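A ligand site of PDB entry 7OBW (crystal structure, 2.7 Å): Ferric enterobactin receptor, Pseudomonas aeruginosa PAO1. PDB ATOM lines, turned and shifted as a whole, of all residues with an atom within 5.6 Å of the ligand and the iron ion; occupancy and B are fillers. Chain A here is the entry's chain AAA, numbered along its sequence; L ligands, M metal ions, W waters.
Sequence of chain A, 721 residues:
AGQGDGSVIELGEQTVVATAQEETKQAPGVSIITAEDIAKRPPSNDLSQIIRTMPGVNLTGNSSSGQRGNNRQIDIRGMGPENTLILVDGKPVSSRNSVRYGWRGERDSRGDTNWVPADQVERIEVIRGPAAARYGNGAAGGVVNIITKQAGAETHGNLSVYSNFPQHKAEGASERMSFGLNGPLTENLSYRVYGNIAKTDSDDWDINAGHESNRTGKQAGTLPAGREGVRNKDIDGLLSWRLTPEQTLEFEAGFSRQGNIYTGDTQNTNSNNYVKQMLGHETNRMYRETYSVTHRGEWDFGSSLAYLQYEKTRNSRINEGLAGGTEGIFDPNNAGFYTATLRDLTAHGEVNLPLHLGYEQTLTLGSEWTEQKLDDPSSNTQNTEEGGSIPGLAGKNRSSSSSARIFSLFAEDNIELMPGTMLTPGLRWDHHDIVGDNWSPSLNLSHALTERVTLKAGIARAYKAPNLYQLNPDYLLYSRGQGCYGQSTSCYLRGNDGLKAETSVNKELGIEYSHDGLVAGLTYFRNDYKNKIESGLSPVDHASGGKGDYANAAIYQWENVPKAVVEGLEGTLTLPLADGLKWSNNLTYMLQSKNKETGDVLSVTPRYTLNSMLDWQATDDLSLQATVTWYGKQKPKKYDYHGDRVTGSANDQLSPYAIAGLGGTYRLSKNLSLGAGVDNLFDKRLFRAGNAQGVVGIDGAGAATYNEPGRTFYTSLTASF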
ATOM      1  N   ARG A 104      18.709 -12.515 -38.404  1.00  0.00           N
ATOM      2  CA  ARG A 104      17.839 -11.859 -39.419  1.00  0.00           C
ATOM      3  C   ARG A 104      18.502 -11.924 -40.812  1.00  0.00           C
ATOM      4  O   ARG A 104      18.040 -11.212 -41.711  1.00  0.00           O
ATOM      5  CB  ARG A 104      17.626 -10.395 -39.009  1.00  0.00           C
ATOM      6  CG  ARG A 104      17.187 -10.217 -37.562  1.00  0.00           C
ATOM      7  CD  ARG A 104      15.974 -11.060 -37.256  1.00  0.00           C
ATOM      8  NE  ARG A 104      15.822 -11.334 -35.830  1.00  0.00           N
ATOM      9  CZ  ARG A 104      14.790 -11.975 -35.302  1.00  0.00           C
ATOM     10  NH1 ARG A 104      13.805 -12.374 -36.089  1.00  0.00           N
ATOM     11  NH2 ARG A 104      14.739 -12.214 -34.000  1.00  0.00           N
ATOM     12  N   LYS A 218      16.991   4.012 -20.902  1.00  0.00           N
ATOM     13  CA  LYS A 218      18.438   3.662 -20.927  1.00  0.00           C
ATOM     14  C   LYS A 218      19.027   3.979 -22.303  1.00  0.00           C
ATOM     15  O   LYS A 218      20.221   4.356 -22.343  1.00  0.00           O
ATOM     16  CB  LYS A 218      18.611   2.214 -20.475  1.00  0.00           C
ATOM     17  CG  LYS A 218      18.199   1.966 -19.029  1.00  0.00           C
ATOM     18  CD  LYS A 218      18.297   0.532 -18.560  1.00  0.00           C
ATOM     19  CE  LYS A 218      17.920   0.390 -17.108  1.00  0.00           C
ATOM     20  NZ  LYS A 218      18.043  -1.017 -16.645  1.00  0.00           N
ATOM     21  N   GLN A 219      18.208   4.022 -23.358  1.00  0.00           N
ATOM     22  CA  GLN A 219      18.689   4.119 -24.768  1.00  0.00           C
ATOM     23  C   GLN A 219      18.694   5.581 -25.235  1.00  0.00           C
ATOM     24  O   GLN A 219      19.101   5.830 -26.397  1.00  0.00           O
ATOM     25  CB  GLN A 219      17.842   3.236 -25.696  1.00  0.00           C
ATOM     26  CG  GLN A 219      17.758   1.774 -25.283  1.00  0.00           C
ATOM     27  CD  GLN A 219      19.079   1.047 -25.276  1.00  0.00           C
ATOM     28  OE1 GLN A 219      20.113   1.562 -25.712  1.00  0.00           O
ATOM     29  NE2 GLN A 219      19.074  -0.164 -24.751  1.00  0.00           N
ATOM     30  N   ASN A 268      21.748  -3.412 -33.206  1.00  0.00           N
ATOM     31  CA  ASN A 268      20.429  -2.924 -32.718  1.00  0.00           C
ATOM     32  C   ASN A 268      20.449  -1.411 -32.497  1.00  0.00           C
ATOM     33  O   ASN A 268      19.369  -0.849 -32.260  1.00  0.00           O
ATOM     34  CB  ASN A 268      19.982  -3.706 -31.480  1.00  0.00           C
ATOM     35  CG  ASN A 268      19.663  -5.142 -31.825  1.00  0.00           C
ATOM     36  OD1 ASN A 268      20.411  -6.051 -31.475  1.00  0.00           O
ATOM     37  ND2 ASN A 268      18.621  -5.337 -32.613  1.00  0.00           N
ATOM     38  N   ASN A 270      22.100   0.133 -30.159  1.00  0.00           N
ATOM     39  CA  ASN A 270      22.510   0.381 -28.752  1.00  0.00           C
ATOM     40  C   ASN A 270      23.969   0.852 -28.739  1.00  0.00           C
ATOM     41  O   ASN A 270      24.624   0.773 -29.783  1.00  0.00           O
ATOM     42  CB  ASN A 270      22.316  -0.848 -27.851  1.00  0.00           C
ATOM     43  CG  ASN A 270      22.592  -2.184 -28.523  1.00  0.00           C
ATOM     44  OD1 ASN A 270      23.106  -2.256 -29.633  1.00  0.00           O
ATOM     45  ND2 ASN A 270      22.264  -3.261 -27.831  1.00  0.00           N
ATOM     46  N   ALA A 323      23.496 -12.783 -28.067  1.00  0.00           N
ATOM     47  CA  ALA A 323      22.212 -12.895 -27.331  1.00  0.00           C
ATOM     48  C   ALA A 323      21.467 -11.548 -27.340  1.00  0.00           C
ATOM     49  O   ALA A 323      21.927 -10.594 -26.641  1.00  0.00           O
ATOM     50  CB  ALA A 323      22.455 -13.385 -25.925  1.00  0.00           C
ATOM     51  N   GLY A 324      20.262 -11.553 -27.913  1.00  0.00           N
ATOM     52  CA  GLY A 324      19.262 -10.464 -27.813  1.00  0.00           C
ATOM     53  C   GLY A 324      19.833  -9.137 -28.279  1.00  0.00           C
ATOM     54  O   GLY A 324      20.321  -9.069 -29.424  1.00  0.00           O
ATOM     55  N   GLY A 325      19.697  -8.117 -27.433  1.00  0.00           N
ATOM     56  CA  GLY A 325      20.276  -6.774 -27.653  1.00  0.00           C
ATOM     57  C   GLY A 325      21.796  -6.778 -27.605  1.00  0.00           C
ATOM     58  O   GLY A 325      22.387  -5.752 -28.020  1.00  0.00           O
ATOM     59  N   THR A 326      22.422  -7.873 -27.145  1.00  0.00           N
ATOM     60  CA  THR A 326      23.906  -7.970 -27.115  1.00  0.00           C
ATOM     61  C   THR A 326      24.428  -8.628 -28.390  1.00  0.00           C
ATOM     62  O   THR A 326      25.672  -8.697 -28.558  1.00  0.00           O
ATOM     63  CB  THR A 326      24.430  -8.656 -25.836  1.00  0.00           C
ATOM     64  OG1 THR A 326      24.133 -10.054 -25.902  1.00  0.00           O
ATOM     65  CG2 THR A 326      23.863  -8.069 -24.570  1.00  0.00           C
ATOM     66  N   GLU A 386      21.581 -19.658 -18.871  1.00  0.00           N
ATOM     67  CA  GLU A 386      20.378 -18.841 -18.610  1.00  0.00           C
ATOM     68  C   GLU A 386      19.148 -19.568 -19.173  1.00  0.00           C
ATOM     69  O   GLU A 386      18.083 -19.366 -18.619  1.00  0.00           O
ATOM     70  CB  GLU A 386      20.544 -17.456 -19.236  1.00  0.00           C
ATOM     71  CG  GLU A 386      19.511 -16.444 -18.760  1.00  0.00           C
ATOM     72  CD  GLU A 386      19.959 -14.992 -18.904  1.00  0.00           C
ATOM     73  OE1 GLU A 386      21.032 -14.652 -18.372  1.00  0.00           O
ATOM     74  OE2 GLU A 386      19.238 -14.207 -19.572  1.00  0.00           O
ATOM     75  N   TYR A 478      20.604 -16.680 -28.824  1.00  0.00           N
ATOM     76  CA  TYR A 478      19.701 -16.718 -27.653  1.00  0.00           C
ATOM     77  C   TYR A 478      19.018 -15.358 -27.501  1.00  0.00           C
ATOM     78  O   TYR A 478      19.674 -14.324 -27.695  1.00  0.00           O
ATOM     79  CB  TYR A 478      20.488 -17.125 -26.398  1.00  0.00           C
ATOM     80  CG  TYR A 478      19.732 -16.986 -25.094  1.00  0.00           C
ATOM     81  CD1 TYR A 478      18.629 -17.773 -24.825  1.00  0.00           C
ATOM     82  CD2 TYR A 478      20.127 -16.074 -24.138  1.00  0.00           C
ATOM     83  CE1 TYR A 478      17.917 -17.640 -23.635  1.00  0.00           C
ATOM     84  CE2 TYR A 478      19.442 -15.927 -22.944  1.00  0.00           C
ATOM     85  CZ  TYR A 478      18.326 -16.707 -22.692  1.00  0.00           C
ATOM     86  OH  TYR A 478      17.613 -16.543 -21.546  1.00  0.00           O
ATOM     87  N   SER A 479      17.714 -15.386 -27.214  1.00  0.00           N
ATOM     88  CA  SER A 479      16.917 -14.196 -26.844  1.00  0.00           C
ATOM     89  C   SER A 479      16.036 -14.561 -25.645  1.00  0.00           C
ATOM     90  O   SER A 479      15.645 -15.735 -25.535  1.00  0.00           O
ATOM     91  CB  SER A 479      16.098 -13.708 -28.006  1.00  0.00           C
ATOM     92  OG  SER A 479      15.168 -12.727 -27.590  1.00  0.00           O
ATOM     93  N   ARG A 480      15.864 -13.597 -24.744  1.00  0.00           N
ATOM     94  CA  ARG A 480      14.984 -13.708 -23.555  1.00  0.00           C
ATOM     95  C   ARG A 480      13.510 -13.610 -23.970  1.00  0.00           C
ATOM     96  O   ARG A 480      12.651 -13.691 -23.075  1.00  0.00           O
ATOM     97  CB  ARG A 480      15.343 -12.598 -22.554  1.00  0.00           C
ATOM     98  CG  ARG A 480      16.638 -12.848 -21.783  1.00  0.00           C
ATOM     99  CD  ARG A 480      17.211 -11.597 -21.121  1.00  0.00           C
ATOM    100  NE  ARG A 480      18.420 -11.881 -20.344  1.00  0.00           N
ATOM    101  CZ  ARG A 480      19.303 -10.971 -19.943  1.00  0.00           C
ATOM    102  NH1 ARG A 480      19.132  -9.686 -20.238  1.00  0.00           N
ATOM    103  NH2 ARG A 480      20.384 -11.347 -19.279  1.00  0.00           N
ATOM    104  N   GLY A 481      13.228 -13.299 -25.241  1.00  0.00           N
ATOM    105  CA  GLY A 481      11.854 -13.244 -25.765  1.00  0.00           C
ATOM    106  C   GLY A 481      11.692 -12.238 -26.883  1.00  0.00           C
ATOM    107  O   GLY A 481      10.925 -12.553 -27.805  1.00  0.00           O
ATOM    108  N   GLN A 482      12.368 -11.080 -26.803  1.00  0.00           N
ATOM    109  CA  GLN A 482      12.048  -9.888 -27.647  1.00  0.00           C
ATOM    110  C   GLN A 482      12.235 -10.217 -29.144  1.00  0.00           C
ATOM    111  O   GLN A 482      11.535  -9.592 -29.964  1.00  0.00           O
ATOM    112  CB  GLN A 482      12.870  -8.671 -27.239  1.00  0.00           C
ATOM    113  CG  GLN A 482      12.642  -7.458 -28.133  1.00  0.00           C
ATOM    114  CD  GLN A 482      13.050  -6.150 -27.500  1.00  0.00           C
ATOM    115  OE1 GLN A 482      12.399  -5.123 -27.682  1.00  0.00           O
ATOM    116  NE2 GLN A 482      14.159  -6.157 -26.774  1.00  0.00           N
ATOM    117  N   GLY A 483      13.060 -11.211 -29.481  1.00  0.00           N
ATOM    118  CA  GLY A 483      13.279 -11.656 -30.869  1.00  0.00           C
ATOM    119  C   GLY A 483      12.736 -13.049 -31.161  1.00  0.00           C
ATOM    120  O   GLY A 483      13.183 -13.669 -32.153  1.00  0.00           O
ATOM    121  N   SER A 488       6.758 -14.526 -26.037  1.00  0.00           N
ATOM    122  CA  SER A 488       7.665 -13.551 -25.342  1.00  0.00           C
ATOM    123  C   SER A 488       8.690 -14.276 -24.467  1.00  0.00           C
ATOM    124  O   SER A 488       9.468 -13.570 -23.800  1.00  0.00           O
ATOM    125  CB  SER A 488       6.866 -12.554 -24.532  1.00  0.00           C
ATOM    126  OG  SER A 488       6.484 -11.468 -25.352  1.00  0.00           O
ATOM    127  N   TYR A 641       9.629  -9.400 -34.973  1.00  0.00           N
ATOM    128  CA  TYR A 641      10.305 -10.709 -34.780  1.00  0.00           C
ATOM    129  C   TYR A 641       9.316 -11.723 -34.183  1.00  0.00           C
ATOM    130  O   TYR A 641       9.387 -12.935 -34.533  1.00  0.00           O
ATOM    131  CB  TYR A 641      11.547 -10.541 -33.896  1.00  0.00           C
ATOM    132  CG  TYR A 641      12.512  -9.471 -34.341  1.00  0.00           C
ATOM    133  CD1 TYR A 641      12.932  -9.379 -35.659  1.00  0.00           C
ATOM    134  CD2 TYR A 641      13.053  -8.583 -33.432  1.00  0.00           C
ATOM    135  CE1 TYR A 641      13.840  -8.410 -36.064  1.00  0.00           C
ATOM    136  CE2 TYR A 641      13.928  -7.579 -33.818  1.00  0.00           C
ATOM    137  CZ  TYR A 641      14.330  -7.504 -35.136  1.00  0.00           C
ATOM    138  OH  TYR A 641      15.213  -6.526 -35.509  1.00  0.00           O
ATOM    139  N   VAL A 695      12.269  -1.745 -30.817  1.00  0.00           N
ATOM    140  CA  VAL A 695      12.617  -2.490 -29.561  1.00  0.00           C
ATOM    141  C   VAL A 695      12.333  -1.590 -28.350  1.00  0.00           C
ATOM    142  O   VAL A 695      11.995  -0.406 -28.528  1.00  0.00           O
ATOM    143  CB  VAL A 695      14.076  -2.988 -29.594  1.00  0.00           C
ATOM    144  CG1 VAL A 695      14.296  -3.962 -30.732  1.00  0.00           C
ATOM    145  CG2 VAL A 695      15.071  -1.842 -29.659  1.00  0.00           C
ATOM    146  N   VAL A 696      12.583  -2.111 -27.138  1.00  0.00           N
ATOM    147  CA  VAL A 696      12.452  -1.356 -25.867  1.00  0.00           C
ATOM    148  C   VAL A 696      13.431  -0.163 -25.892  1.00  0.00           C
ATOM    149  O   VAL A 696      14.651  -0.408 -25.953  1.00  0.00           O
ATOM    150  CB  VAL A 696      12.714  -2.271 -24.652  1.00  0.00           C
ATOM    151  CG1 VAL A 696      12.927  -1.463 -23.370  1.00  0.00           C
ATOM    152  CG2 VAL A 696      11.605  -3.291 -24.465  1.00  0.00           C
ATOM    153  N   ILE A 698      14.020   2.035 -28.145  1.00  0.00           N
ATOM    154  CA  ILE A 698      14.423   2.400 -29.539  1.00  0.00           C
ATOM    155  C   ILE A 698      13.230   2.168 -30.471  1.00  0.00           C
ATOM    156  O   ILE A 698      13.118   1.059 -30.991  1.00  0.00           O
ATOM    157  CB  ILE A 698      15.676   1.636 -29.996  1.00  0.00           C
ATOM    158  CG1 ILE A 698      16.750   1.598 -28.904  1.00  0.00           C
ATOM    159  CG2 ILE A 698      16.217   2.231 -31.293  1.00  0.00           C
ATOM    160  CD1 ILE A 698      17.891   0.656 -29.199  1.00  0.00           C
HETATM  161  C1  LIG L   1      13.672  -9.693 -24.200  1.00  0.00           C
HETATM  162  C2  LIG L   1      12.406 -10.104 -23.791  1.00  0.00           C
HETATM  163  C3  LIG L   1      11.662  -9.338 -22.903  1.00  0.00           C
HETATM  164  C4  LIG L   1      12.190  -8.142 -22.420  1.00  0.00           C
HETATM  165  C5  LIG L   1      17.850  -0.700 -21.729  1.00  0.00           C
HETATM  166  C6  LIG L   1      14.194  -8.484 -23.719  1.00  0.00           C
HETATM  167  O1  LIG L   1      17.472  -4.549 -29.196  1.00  0.00           O
HETATM  168  C7  LIG L   1      17.115  -5.404 -28.385  1.00  0.00           C
HETATM  169  C8  LIG L   1      16.801  -6.798 -28.872  1.00  0.00           C
HETATM  170  C9  LIG L   1      16.526  -7.829 -27.975  1.00  0.00           C
HETATM  171  O2  LIG L   1      16.535  -7.566 -26.627  1.00  0.00           O
HETATM  172  C10 LIG L   1      16.257  -9.115 -28.427  1.00  0.00           C
HETATM  173  O3  LIG L   1      15.985 -10.132 -27.549  1.00  0.00           O
HETATM  174  C11 LIG L   1      16.260  -9.385 -29.803  1.00  0.00           C
HETATM  175  C12 LIG L   1      16.533  -8.364 -30.702  1.00  0.00           C
HETATM  176  C13 LIG L   1      16.798  -7.078 -30.241  1.00  0.00           C
HETATM  177  N1  LIG L   1      17.050  -5.123 -27.088  1.00  0.00           N
HETATM  178  C14 LIG L   1      17.432  -3.825 -26.572  1.00  0.00           C
HETATM  179  C15 LIG L   1      18.806  -3.862 -25.944  1.00  0.00           C
HETATM  180  O4  LIG L   1      19.691  -3.106 -26.314  1.00  0.00           O
HETATM  181  N2  LIG L   1      18.993  -4.746 -24.973  1.00  0.00           N
HETATM  182  C16 LIG L   1      20.271  -4.836 -24.288  1.00  0.00           C
HETATM  183  C17 LIG L   1      20.155  -5.636 -22.995  1.00  0.00           C
HETATM  184  N3  LIG L   1      19.909  -7.036 -23.296  1.00  0.00           N
HETATM  185  C18 LIG L   1      20.781  -8.005 -22.998  1.00  0.00           C
HETATM  186  C19 LIG L   1      20.329  -9.418 -23.253  1.00  0.00           C
HETATM  187  C20 LIG L   1      19.168  -9.607 -23.991  1.00  0.00           C
HETATM  188  O5  LIG L   1      18.464  -8.518 -24.438  1.00  0.00           O
HETATM  189  C21 LIG L   1      18.731 -10.905 -24.263  1.00  0.00           C
HETATM  190  O6  LIG L   1      17.554 -11.082 -24.940  1.00  0.00           O
HETATM  191  C22 LIG L   1      19.463 -12.011 -23.814  1.00  0.00           C
HETATM  192  C23 LIG L   1      20.649 -11.814 -23.095  1.00  0.00           C
HETATM  193  C24 LIG L   1      21.087 -10.516 -22.824  1.00  0.00           C
HETATM  194  O7  LIG L   1      21.902  -7.811 -22.522  1.00  0.00           O
HETATM  195  C25 LIG L   1      19.061  -5.028 -22.154  1.00  0.00           C
HETATM  196  N4  LIG L   1      18.111  -5.846 -21.678  1.00  0.00           N
HETATM  197  C26 LIG L   1      17.045  -5.374 -20.824  1.00  0.00           C
HETATM  198  C27 LIG L   1      15.793  -4.961 -21.613  1.00  0.00           C
HETATM  199  N5  LIG L   1      15.265  -6.105 -22.332  1.00  0.00           N
HETATM  200  C28 LIG L   1      13.962  -6.402 -22.300  1.00  0.00           C
HETATM  201  O8  LIG L   1      13.154  -5.622 -21.824  1.00  0.00           O
HETATM  202  C29 LIG L   1      16.052  -3.752 -22.491  1.00  0.00           C
HETATM  203  O9  LIG L   1      15.881  -3.807 -23.702  1.00  0.00           O
HETATM  204  N6  LIG L   1      16.431  -2.640 -21.846  1.00  0.00           N
HETATM  205  C30 LIG L   1      16.771  -1.392 -22.515  1.00  0.00           C
HETATM  206  O10 LIG L   1      19.064  -3.823 -21.949  1.00  0.00           O
HETATM  207  C31 LIG L   1      13.460  -7.721 -22.826  1.00  0.00           C
HETATM  208  O11 LIG L   1      15.422  -8.044 -24.123  1.00  0.00           O
HETATM  209  O12 LIG L   1      14.349 -10.472 -25.103  1.00  0.00           O
HETATM  210 FE    FE M   1      16.584  -9.254 -25.303  1.00  0.00          FE
HETATM  211  O   HOH W   1      17.135  -8.492 -21.559  1.00  0.00           O
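O5 of the ligand lies close to N of Gly 325 (3.3 Å). The backbone NH (N) of Gln 482 lies close to an oxygen (O12) of the ligand, 2.7 Å away. OG of Ser 479 lies close to O3 of the ligand (2.7 Å). N1 of the ligand lies close to NE2 of Gln 482 (3.1 Å). The backbone NH of Arg 480 sits close to an oxygen (O6) of the ligand (3.0 Å). The side-chain amide nitrogen (NE2) of Gln 219 lies close to an oxygen (O4) of the ligand (3.4 Å). An oxygen (O4) of the ligand sits at hydrogen-bond distance from the side-chain amide nitrogen (ND2) of Asn 270, at 3.0 Å. The backbone NH (N) of Gly 481 lies close to an oxygen (O12) of the ligand (3.0 Å).
N of Gln 482 sits at hydrogen-bond distance from OG of Ser 479 (3.3 Å). O of Gly 325 is in hydrogen-bond range of ND2 of Asn 270 (2.5 Å). The backbone NH (N) of Gly 481 is in hydrogen-bond range of the side-chain hydroxyl (OG) of Ser 479. The guanidinium group (NE) of Arg 480 is in salt-bridge range of the side-chain carboxylate (OE2) of Glu 386 (2.6 Å). The side-chain hydroxyl of Ser 479 is in hydrogen-bond range of the backbone NH of Gly 483 (3.2 Å). The side-chain amide oxygen (OE1) of Gln 482 lies within hydrogen-bond range of the backbone NH (N) of Val 696 (3.1 Å). N of Gly 324 is in hydrogen-bond range of O of Tyr 478 (2.8 Å). The backbone carbonyl oxygen (O) of Gly 483 sits at hydrogen-bond distance from the guanidinium group (NH2) of Arg 104, at 2.8 Å.
Merely in contact with the ligand: Thr 326, Lys 218, Gly 324, Asn 268, Val 695, Val 696, Gly 483 and Ala 323. Hydrophobic or aromatic side chains that line the ligand: Ala 323, Val 695 and Val 696.
Merely in contact with the iron ion: Gly 324 (3.9 Å) and Gly 325 (3.9 Å). Of the 21 residues printed, 2 come within 4 Å of the iron ion.
The iron ion is bound by an oxygen (O11) of the ligand (2.1 Å), an oxygen (O6) of the ligand (2.1 Å), an oxygen (O2) of the ligand (2.1 Å), an oxygen (O5) of the ligand (2.2 Å), an oxygen (O3) of the ligand (2.5 Å) and an oxygen (O12) of the ligand (2.6 Å).
Water W1 bridges NH1 of Arg 480 (2.7 Å) and N4 of the ligand (2.8 Å).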
